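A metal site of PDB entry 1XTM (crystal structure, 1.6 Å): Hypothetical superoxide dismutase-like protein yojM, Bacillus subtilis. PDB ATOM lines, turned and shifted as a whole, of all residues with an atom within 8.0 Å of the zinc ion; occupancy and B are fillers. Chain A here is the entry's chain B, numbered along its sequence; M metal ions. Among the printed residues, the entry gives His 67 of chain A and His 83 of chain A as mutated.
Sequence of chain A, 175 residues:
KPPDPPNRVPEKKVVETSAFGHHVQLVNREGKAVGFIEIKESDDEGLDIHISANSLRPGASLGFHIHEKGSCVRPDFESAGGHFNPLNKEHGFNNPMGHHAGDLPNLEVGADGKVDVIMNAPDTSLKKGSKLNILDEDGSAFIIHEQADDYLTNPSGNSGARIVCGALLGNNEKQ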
ATOM      1  N   PHE A  64      21.338  -8.515  20.647  1.00  0.00           N
ATOM      2  CA  PHE A  64      22.238  -9.552  20.234  1.00  0.00           C
ATOM      3  C   PHE A  64      23.671  -9.068  20.427  1.00  0.00           C
ATOM      4  O   PHE A  64      24.081  -8.068  19.822  1.00  0.00           O
ATOM      5  CB  PHE A  64      22.031  -9.855  18.755  1.00  0.00           C
ATOM      6  CG  PHE A  64      22.871 -11.010  18.239  1.00  0.00           C
ATOM      7  CD1 PHE A  64      23.069 -12.188  19.026  1.00  0.00           C
ATOM      8  CD2 PHE A  64      23.353 -10.990  16.901  1.00  0.00           C
ATOM      9  CE1 PHE A  64      23.814 -13.254  18.500  1.00  0.00           C
ATOM     10  CE2 PHE A  64      24.078 -12.081  16.375  1.00  0.00           C
ATOM     11  CZ  PHE A  64      24.303 -13.220  17.177  1.00  0.00           C
ATOM     12  N   HIS A  65      24.418  -9.794  21.259  1.00  0.00           N
ATOM     13  CA  HIS A  65      25.757  -9.348  21.698  1.00  0.00           C
ATOM     14  C   HIS A  65      26.696 -10.492  21.880  1.00  0.00           C
ATOM     15  O   HIS A  65      26.262 -11.609  22.325  1.00  0.00           O
ATOM     16  CB  HIS A  65      25.747  -8.634  23.078  1.00  0.00           C
ATOM     17  CG  HIS A  65      24.599  -7.686  23.281  1.00  0.00           C
ATOM     18  ND1 HIS A  65      23.783  -7.746  24.390  1.00  0.00           N
ATOM     19  CD2 HIS A  65      24.169  -6.619  22.555  1.00  0.00           C
ATOM     20  CE1 HIS A  65      22.877  -6.786  24.320  1.00  0.00           C
ATOM     21  NE2 HIS A  65      23.087  -6.087  23.222  1.00  0.00           N
ATOM     22  N   ILE A  66      27.971 -10.225  21.642  1.00  0.00           N
ATOM     23  CA  ILE A  66      29.011 -11.154  22.048  1.00  0.00           C
ATOM     24  C   ILE A  66      29.425 -10.775  23.460  1.00  0.00           C
ATOM     25  O   ILE A  66      29.815  -9.610  23.756  1.00  0.00           O
ATOM     26  CB  ILE A  66      30.256 -11.161  21.101  1.00  0.00           C
ATOM     27  CG1 ILE A  66      29.829 -11.446  19.659  1.00  0.00           C
ATOM     28  CG2 ILE A  66      31.261 -12.222  21.577  1.00  0.00           C
ATOM     29  CD1 ILE A  66      30.933 -11.196  18.595  1.00  0.00           C
ATOM     30  N   HIS A  67      29.303 -11.749  24.367  1.00  0.00           N
ATOM     31  CA  HIS A  67      29.677 -11.558  25.772  1.00  0.00           C
ATOM     32  C   HIS A  67      31.096 -12.146  26.046  1.00  0.00           C
ATOM     33  O   HIS A  67      31.594 -12.989  25.277  1.00  0.00           O
ATOM     34  CB  HIS A  67      28.621 -12.193  26.697  1.00  0.00           C
ATOM     35  CG  HIS A  67      27.350 -11.401  26.774  1.00  0.00           C
ATOM     36  ND1 HIS A  67      26.893 -10.852  27.958  1.00  0.00           N
ATOM     37  CD2 HIS A  67      26.476 -11.003  25.822  1.00  0.00           C
ATOM     38  CE1 HIS A  67      25.762 -10.204  27.742  1.00  0.00           C
ATOM     39  NE2 HIS A  67      25.492 -10.284  26.447  1.00  0.00           N
ATOM     40  N   GLY A  82      30.140  -9.975  30.747  1.00  0.00           N
ATOM     41  CA  GLY A  82      29.605  -8.632  30.564  1.00  0.00           C
ATOM     42  C   GLY A  82      29.735  -8.623  28.998  1.00  0.00           C
ATOM     43  O   GLY A  82      30.187  -9.619  28.424  1.00  0.00           O
ATOM     44  N   HIS A  83      29.350  -7.561  28.281  1.00  0.00           N
ATOM     45  CA  HIS A  83      29.589  -7.485  26.830  1.00  0.00           C
ATOM     46  C   HIS A  83      31.111  -7.451  26.553  1.00  0.00           C
ATOM     47  O   HIS A  83      31.860  -6.859  27.349  1.00  0.00           O
ATOM     48  CB  HIS A  83      29.004  -6.194  26.234  1.00  0.00           C
ATOM     49  CG  HIS A  83      27.515  -6.102  26.264  1.00  0.00           C
ATOM     50  ND1 HIS A  83      26.812  -5.069  25.662  1.00  0.00           N
ATOM     51  CD2 HIS A  83      26.579  -6.927  26.807  1.00  0.00           C
ATOM     52  CE1 HIS A  83      25.515  -5.261  25.844  1.00  0.00           C
ATOM     53  NE2 HIS A  83      25.347  -6.377  26.517  1.00  0.00           N
ATOM     54  N   PHE A  84      31.552  -8.067  25.468  1.00  0.00           N
ATOM     55  CA  PHE A  84      32.979  -8.172  25.130  1.00  0.00           C
ATOM     56  C   PHE A  84      33.407  -6.734  24.820  1.00  0.00           C
ATOM     57  O   PHE A  84      32.806  -6.091  23.948  1.00  0.00           O
ATOM     58  CB  PHE A  84      33.159  -9.078  23.915  1.00  0.00           C
ATOM     59  CG  PHE A  84      34.569  -9.132  23.371  1.00  0.00           C
ATOM     60  CD1 PHE A  84      34.815  -8.860  22.012  1.00  0.00           C
ATOM     61  CD2 PHE A  84      35.630  -9.532  24.168  1.00  0.00           C
ATOM     62  CE1 PHE A  84      36.122  -8.947  21.479  1.00  0.00           C
ATOM     63  CE2 PHE A  84      36.943  -9.612  23.631  1.00  0.00           C
ATOM     64  CZ  PHE A  84      37.166  -9.322  22.268  1.00  0.00           C
ATOM     65  N   ASN A  85      34.396  -6.252  25.566  1.00  0.00           N
ATOM     66  CA  ASN A  85      34.750  -4.792  25.585  1.00  0.00           C
ATOM     67  C   ASN A  85      36.266  -4.538  25.753  1.00  0.00           C
ATOM     68  O   ASN A  85      36.692  -3.850  26.728  1.00  0.00           O
ATOM     69  CB  ASN A  85      33.968  -4.129  26.730  1.00  0.00           C
ATOM     70  CG  ASN A  85      33.990  -2.589  26.679  1.00  0.00           C
ATOM     71  OD1 ASN A  85      34.242  -1.974  25.627  1.00  0.00           O
ATOM     72  ND2 ASN A  85      33.700  -1.979  27.815  1.00  0.00           N
ATOM     73  N   LYS A  89      34.967   0.828  26.031  1.00  0.00           N
ATOM     74  CA  LYS A  89      33.936   1.817  25.689  1.00  0.00           C
ATOM     75  C   LYS A  89      32.604   1.566  26.436  1.00  0.00           C
ATOM     76  O   LYS A  89      32.461   0.557  27.155  1.00  0.00           O
ATOM     77  CB  LYS A  89      33.724   1.865  24.165  1.00  0.00           C
ATOM     78  CG  LYS A  89      34.991   1.646  23.340  1.00  0.00           C
ATOM     79  CD  LYS A  89      34.898   2.163  21.931  1.00  0.00           C
ATOM     80  CE  LYS A  89      35.553   3.551  21.786  1.00  0.00           C
ATOM     81  NZ  LYS A  89      35.070   4.218  20.523  1.00  0.00           N
ATOM     82  N   GLU A  90      31.661   2.511  26.290  1.00  0.00           N
ATOM     83  CA  GLU A  90      30.293   2.379  26.798  1.00  0.00           C
ATOM     84  C   GLU A  90      29.480   1.592  25.799  1.00  0.00           C
ATOM     85  O   GLU A  90      29.961   1.277  24.702  1.00  0.00           O
ATOM     86  CB  GLU A  90      29.657   3.757  27.016  1.00  0.00           C
ATOM     87  CG  GLU A  90      30.234   4.552  28.184  1.00  0.00           C
ATOM     88  CD  GLU A  90      29.410   5.789  28.511  1.00  0.00           C
ATOM     89  OE1 GLU A  90      28.295   5.948  27.940  1.00  0.00           O
ATOM     90  OE2 GLU A  90      29.882   6.622  29.337  1.00  0.00           O
ATOM     91  N   HIS A  91      28.243   1.251  26.164  1.00  0.00           N
ATOM     92  CA  HIS A  91      27.395   0.532  25.230  1.00  0.00           C
ATOM     93  C   HIS A  91      26.784   1.414  24.129  1.00  0.00           C
ATOM     94  O   HIS A  91      26.343   2.525  24.387  1.00  0.00           O
ATOM     95  CB  HIS A  91      26.277  -0.201  25.993  1.00  0.00           C
ATOM     96  CG  HIS A  91      25.344  -0.942  25.096  1.00  0.00           C
ATOM     97  ND1 HIS A  91      25.685  -2.155  24.501  1.00  0.00           N
ATOM     98  CD2 HIS A  91      24.118  -0.626  24.620  1.00  0.00           C
ATOM     99  CE1 HIS A  91      24.702  -2.539  23.709  1.00  0.00           C
ATOM    100  NE2 HIS A  91      23.726  -1.642  23.774  1.00  0.00           N
ATOM    101  N   GLY A  92      26.704   0.882  22.907  1.00  0.00           N
ATOM    102  CA  GLY A  92      25.703   1.328  21.950  1.00  0.00           C
ATOM    103  C   GLY A  92      26.184   2.072  20.715  1.00  0.00           C
ATOM    104  O   GLY A  92      26.957   3.038  20.830  1.00  0.00           O
ATOM    105  N   PHE A  93      25.722   1.630  19.542  1.00  0.00           N
ATOM    106  CA  PHE A  93      26.101   2.262  18.260  1.00  0.00           C
ATOM    107  C   PHE A  93      25.743   3.739  18.225  1.00  0.00           C
ATOM    108  O   PHE A  93      26.422   4.487  17.511  1.00  0.00           O
ATOM    109  CB  PHE A  93      25.415   1.632  17.046  1.00  0.00           C
ATOM    110  CG  PHE A  93      25.714   0.164  16.860  1.00  0.00           C
ATOM    111  CD1 PHE A  93      24.671  -0.732  16.706  1.00  0.00           C
ATOM    112  CD2 PHE A  93      27.013  -0.308  16.852  1.00  0.00           C
ATOM    113  CE1 PHE A  93      24.927  -2.100  16.543  1.00  0.00           C
ATOM    114  CE2 PHE A  93      27.274  -1.676  16.667  1.00  0.00           C
ATOM    115  CZ  PHE A  93      26.218  -2.570  16.524  1.00  0.00           C
ATOM    116  N   HIS A  99      31.420   2.155  21.139  1.00  0.00           N
ATOM    117  CA  HIS A  99      30.525   1.065  21.589  1.00  0.00           C
ATOM    118  C   HIS A  99      31.355  -0.172  21.856  1.00  0.00           C
ATOM    119  O   HIS A  99      32.503  -0.275  21.460  1.00  0.00           O
ATOM    120  CB  HIS A  99      29.459   0.733  20.533  1.00  0.00           C
ATOM    121  CG  HIS A  99      29.990   0.494  19.162  1.00  0.00           C
ATOM    122  ND1 HIS A  99      30.096   1.524  18.227  1.00  0.00           N
ATOM    123  CD2 HIS A  99      30.395  -0.628  18.519  1.00  0.00           C
ATOM    124  CE1 HIS A  99      30.546   1.027  17.089  1.00  0.00           C
ATOM    125  NE2 HIS A  99      30.743  -0.271  17.237  1.00  0.00           N
ATOM    126  N   HIS A 100      30.773  -1.134  22.539  1.00  0.00           N
ATOM    127  CA  HIS A 100      31.481  -2.378  22.746  1.00  0.00           C
ATOM    128  C   HIS A 100      31.783  -3.134  21.478  1.00  0.00           C
ATOM    129  O   HIS A 100      30.940  -3.203  20.576  1.00  0.00           O
ATOM    130  CB  HIS A 100      30.623  -3.263  23.620  1.00  0.00           C
ATOM    131  CG  HIS A 100      30.245  -2.633  24.928  1.00  0.00           C
ATOM    132  ND1 HIS A 100      29.014  -2.800  25.520  1.00  0.00           N
ATOM    133  CD2 HIS A 100      30.963  -1.871  25.775  1.00  0.00           C
ATOM    134  CE1 HIS A 100      28.988  -2.156  26.671  1.00  0.00           C
ATOM    135  NE2 HIS A 100      30.159  -1.587  26.850  1.00  0.00           N
ATOM    136  N   ALA A 101      32.959  -3.735  21.473  1.00  0.00           N
ATOM    137  CA  ALA A 101      33.393  -4.576  20.391  1.00  0.00           C
ATOM    138  C   ALA A 101      32.346  -5.718  20.130  1.00  0.00           C
ATOM    139  O   ALA A 101      32.083  -6.109  18.984  1.00  0.00           O
ATOM    140  CB  ALA A 101      34.751  -5.138  20.704  1.00  0.00           C
ATOM    141  N   GLY A 102      31.725  -6.110  21.216  1.00  0.00           N
ATOM    142  CA  GLY A 102      30.711  -7.211  21.182  1.00  0.00           C
ATOM    143  C   GLY A 102      29.311  -6.756  20.793  1.00  0.00           C
ATOM    144  O   GLY A 102      28.353  -7.582  20.744  1.00  0.00           O
ATOM    145  N   ASP A 103      29.123  -5.460  20.496  1.00  0.00           N
ATOM    146  CA  ASP A 103      27.778  -4.968  20.173  1.00  0.00           C
ATOM    147  C   ASP A 103      27.448  -5.318  18.765  1.00  0.00           C
ATOM    148  O   ASP A 103      28.204  -4.961  17.858  1.00  0.00           O
ATOM    149  CB  ASP A 103      27.586  -3.434  20.400  1.00  0.00           C
ATOM    150  CG  ASP A 103      27.614  -3.070  21.865  1.00  0.00           C
ATOM    151  OD1 ASP A 103      27.713  -1.860  22.216  1.00  0.00           O
ATOM    152  OD2 ASP A 103      27.547  -3.935  22.782  1.00  0.00           O
ATOM    153  N   LEU A 104      26.308  -5.998  18.578  1.00  0.00           N
ATOM    154  CA  LEU A 104      25.891  -6.402  17.229  1.00  0.00           C
ATOM    155  C   LEU A 104      24.487  -5.865  16.928  1.00  0.00           C
ATOM    156  O   LEU A 104      23.799  -5.474  17.870  1.00  0.00           O
ATOM    157  CB  LEU A 104      25.868  -7.929  17.116  1.00  0.00           C
ATOM    158  CG  LEU A 104      27.147  -8.720  17.314  1.00  0.00           C
ATOM    159  CD1 LEU A 104      26.856 -10.238  17.182  1.00  0.00           C
ATOM    160  CD2 LEU A 104      28.251  -8.284  16.335  1.00  0.00           C
ATOM    161  N   ASP A 149      17.680  -4.004  21.693  1.00  0.00           N
ATOM    162  CA  ASP A 149      18.759  -3.148  22.144  1.00  0.00           C
ATOM    163  C   ASP A 149      18.465  -1.716  21.577  1.00  0.00           C
ATOM    164  O   ASP A 149      18.221  -1.574  20.374  1.00  0.00           O
ATOM    165  CB  ASP A 149      20.073  -3.717  21.583  1.00  0.00           C
ATOM    166  CG  ASP A 149      21.328  -3.038  22.151  1.00  0.00           C
ATOM    167  OD1 ASP A 149      21.267  -1.833  22.531  1.00  0.00           O
ATOM    168  OD2 ASP A 149      22.405  -3.668  22.240  1.00  0.00           O
ATOM    169  N   THR A 153      21.655   2.896  25.844  1.00  0.00           N
ATOM    170  CA  THR A 153      21.651   2.829  27.290  1.00  0.00           C
ATOM    171  C   THR A 153      22.720   1.874  27.787  1.00  0.00           C
ATOM    172  O   THR A 153      22.875   0.766  27.270  1.00  0.00           O
ATOM    173  CB  THR A 153      20.263   2.364  27.776  1.00  0.00           C
ATOM    174  OG1 THR A 153      19.275   3.309  27.348  1.00  0.00           O
ATOM    175  CG2 THR A 153      20.172   2.418  29.305  1.00  0.00           C
ATOM    176  N   ASN A 154      23.477   2.305  28.797  1.00  0.00           N
ATOM    177  CA  ASN A 154      24.368   1.412  29.513  1.00  0.00           C
ATOM    178  C   ASN A 154      23.639   0.499  30.480  1.00  0.00           C
ATOM    179  O   ASN A 154      22.577   0.862  31.012  1.00  0.00           O
ATOM    180  CB  ASN A 154      25.413   2.220  30.270  1.00  0.00           C
ATOM    181  CG  ASN A 154      26.504   2.737  29.361  1.00  0.00           C
ATOM    182  OD1 ASN A 154      27.345   1.974  28.870  1.00  0.00           O
ATOM    183  ND2 ASN A 154      26.504   4.045  29.137  1.00  0.00           N
ATOM    184  N   PRO A 155      24.218  -0.691  30.724  1.00  0.00           N
ATOM    185  CA  PRO A 155      25.362  -1.197  29.946  1.00  0.00           C
ATOM    186  C   PRO A 155      24.987  -2.184  28.813  1.00  0.00           C
ATOM    187  O   PRO A 155      25.890  -2.675  28.118  1.00  0.00           O
ATOM    188  CB  PRO A 155      26.189  -1.897  31.028  1.00  0.00           C
ATOM    189  CG  PRO A 155      25.149  -2.436  31.983  1.00  0.00           C
ATOM    190  CD  PRO A 155      23.880  -1.586  31.848  1.00  0.00           C
ATOM    191  N   SER A 156      23.696  -2.477  28.637  1.00  0.00           N
ATOM    192  CA  SER A 156      23.228  -3.443  27.633  1.00  0.00           C
ATOM    193  C   SER A 156      22.081  -2.981  26.717  1.00  0.00           C
ATOM    194  O   SER A 156      21.407  -3.805  26.099  1.00  0.00           O
ATOM    195  CB  SER A 156      22.840  -4.765  28.324  1.00  0.00           C
ATOM    196  OG  SER A 156      22.208  -4.469  29.569  1.00  0.00           O
ATOM    197  N   GLY A 157      21.840  -1.663  26.630  1.00  0.00           N
ATOM    198  CA  GLY A 157      20.818  -1.130  25.742  1.00  0.00           C
ATOM    199  C   GLY A 157      19.398  -1.451  26.150  1.00  0.00           C
ATOM    200  O   GLY A 157      18.484  -1.396  25.340  1.00  0.00           O
ATOM    201  N   SER A 159      18.185  -4.238  26.828  1.00  0.00           N
ATOM    202  CA  SER A 159      17.841  -5.481  26.119  1.00  0.00           C
ATOM    203  C   SER A 159      17.105  -6.502  27.007  1.00  0.00           C
ATOM    204  O   SER A 159      16.538  -7.459  26.509  1.00  0.00           O
ATOM    205  CB  SER A 159      19.110  -6.150  25.523  1.00  0.00           C
ATOM    206  OG  SER A 159      19.802  -5.253  24.639  1.00  0.00           O
HETATM  207 ZN    ZN M   1      27.280  -3.438  24.666  1.00  0.00          ZN
HETATM  208 CU    CU M   2      23.854  -9.138  25.909  1.00  0.00          CU
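N of Gly 92 lies within hydrogen-bond range of OD1 of Asp 103 (3.0 Å).
A ring nitrogen (NE2) of His 83 lies close to a ring nitrogen (ND1) of His 65, at 3.0 Å.
The backbone NH of His 100 sits at hydrogen-bond distance from the backbone carbonyl oxygen of Glu 90 (3.3 Å).
A ring nitrogen (NE2) of His 100 is in hydrogen-bond range of the backbone carbonyl oxygen (O) of Lys 89, 3.2 Å away.
NE2 of His 91 is in hydrogen-bond range of OD1 of Asp 149.
NE2 of His 91 sits close to N of Gly 157 (3.4 Å).
N of His 91 is in hydrogen-bond range of OD1 of Asn 154.
Pro 155 touches the zinc ion.
Of the 26 residues printed, 5 come within 4 Å of the zinc ion.
The zinc ion is bound by the side-chain carboxylate (OD2) of Asp 103 (2.0 Å), a ring nitrogen (ND1) of His 83 (2.0 Å), a ring nitrogen (ND1) of His 100 (2.0 Å) and a ring nitrogen (ND1) of His 91 (2.1 Å).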
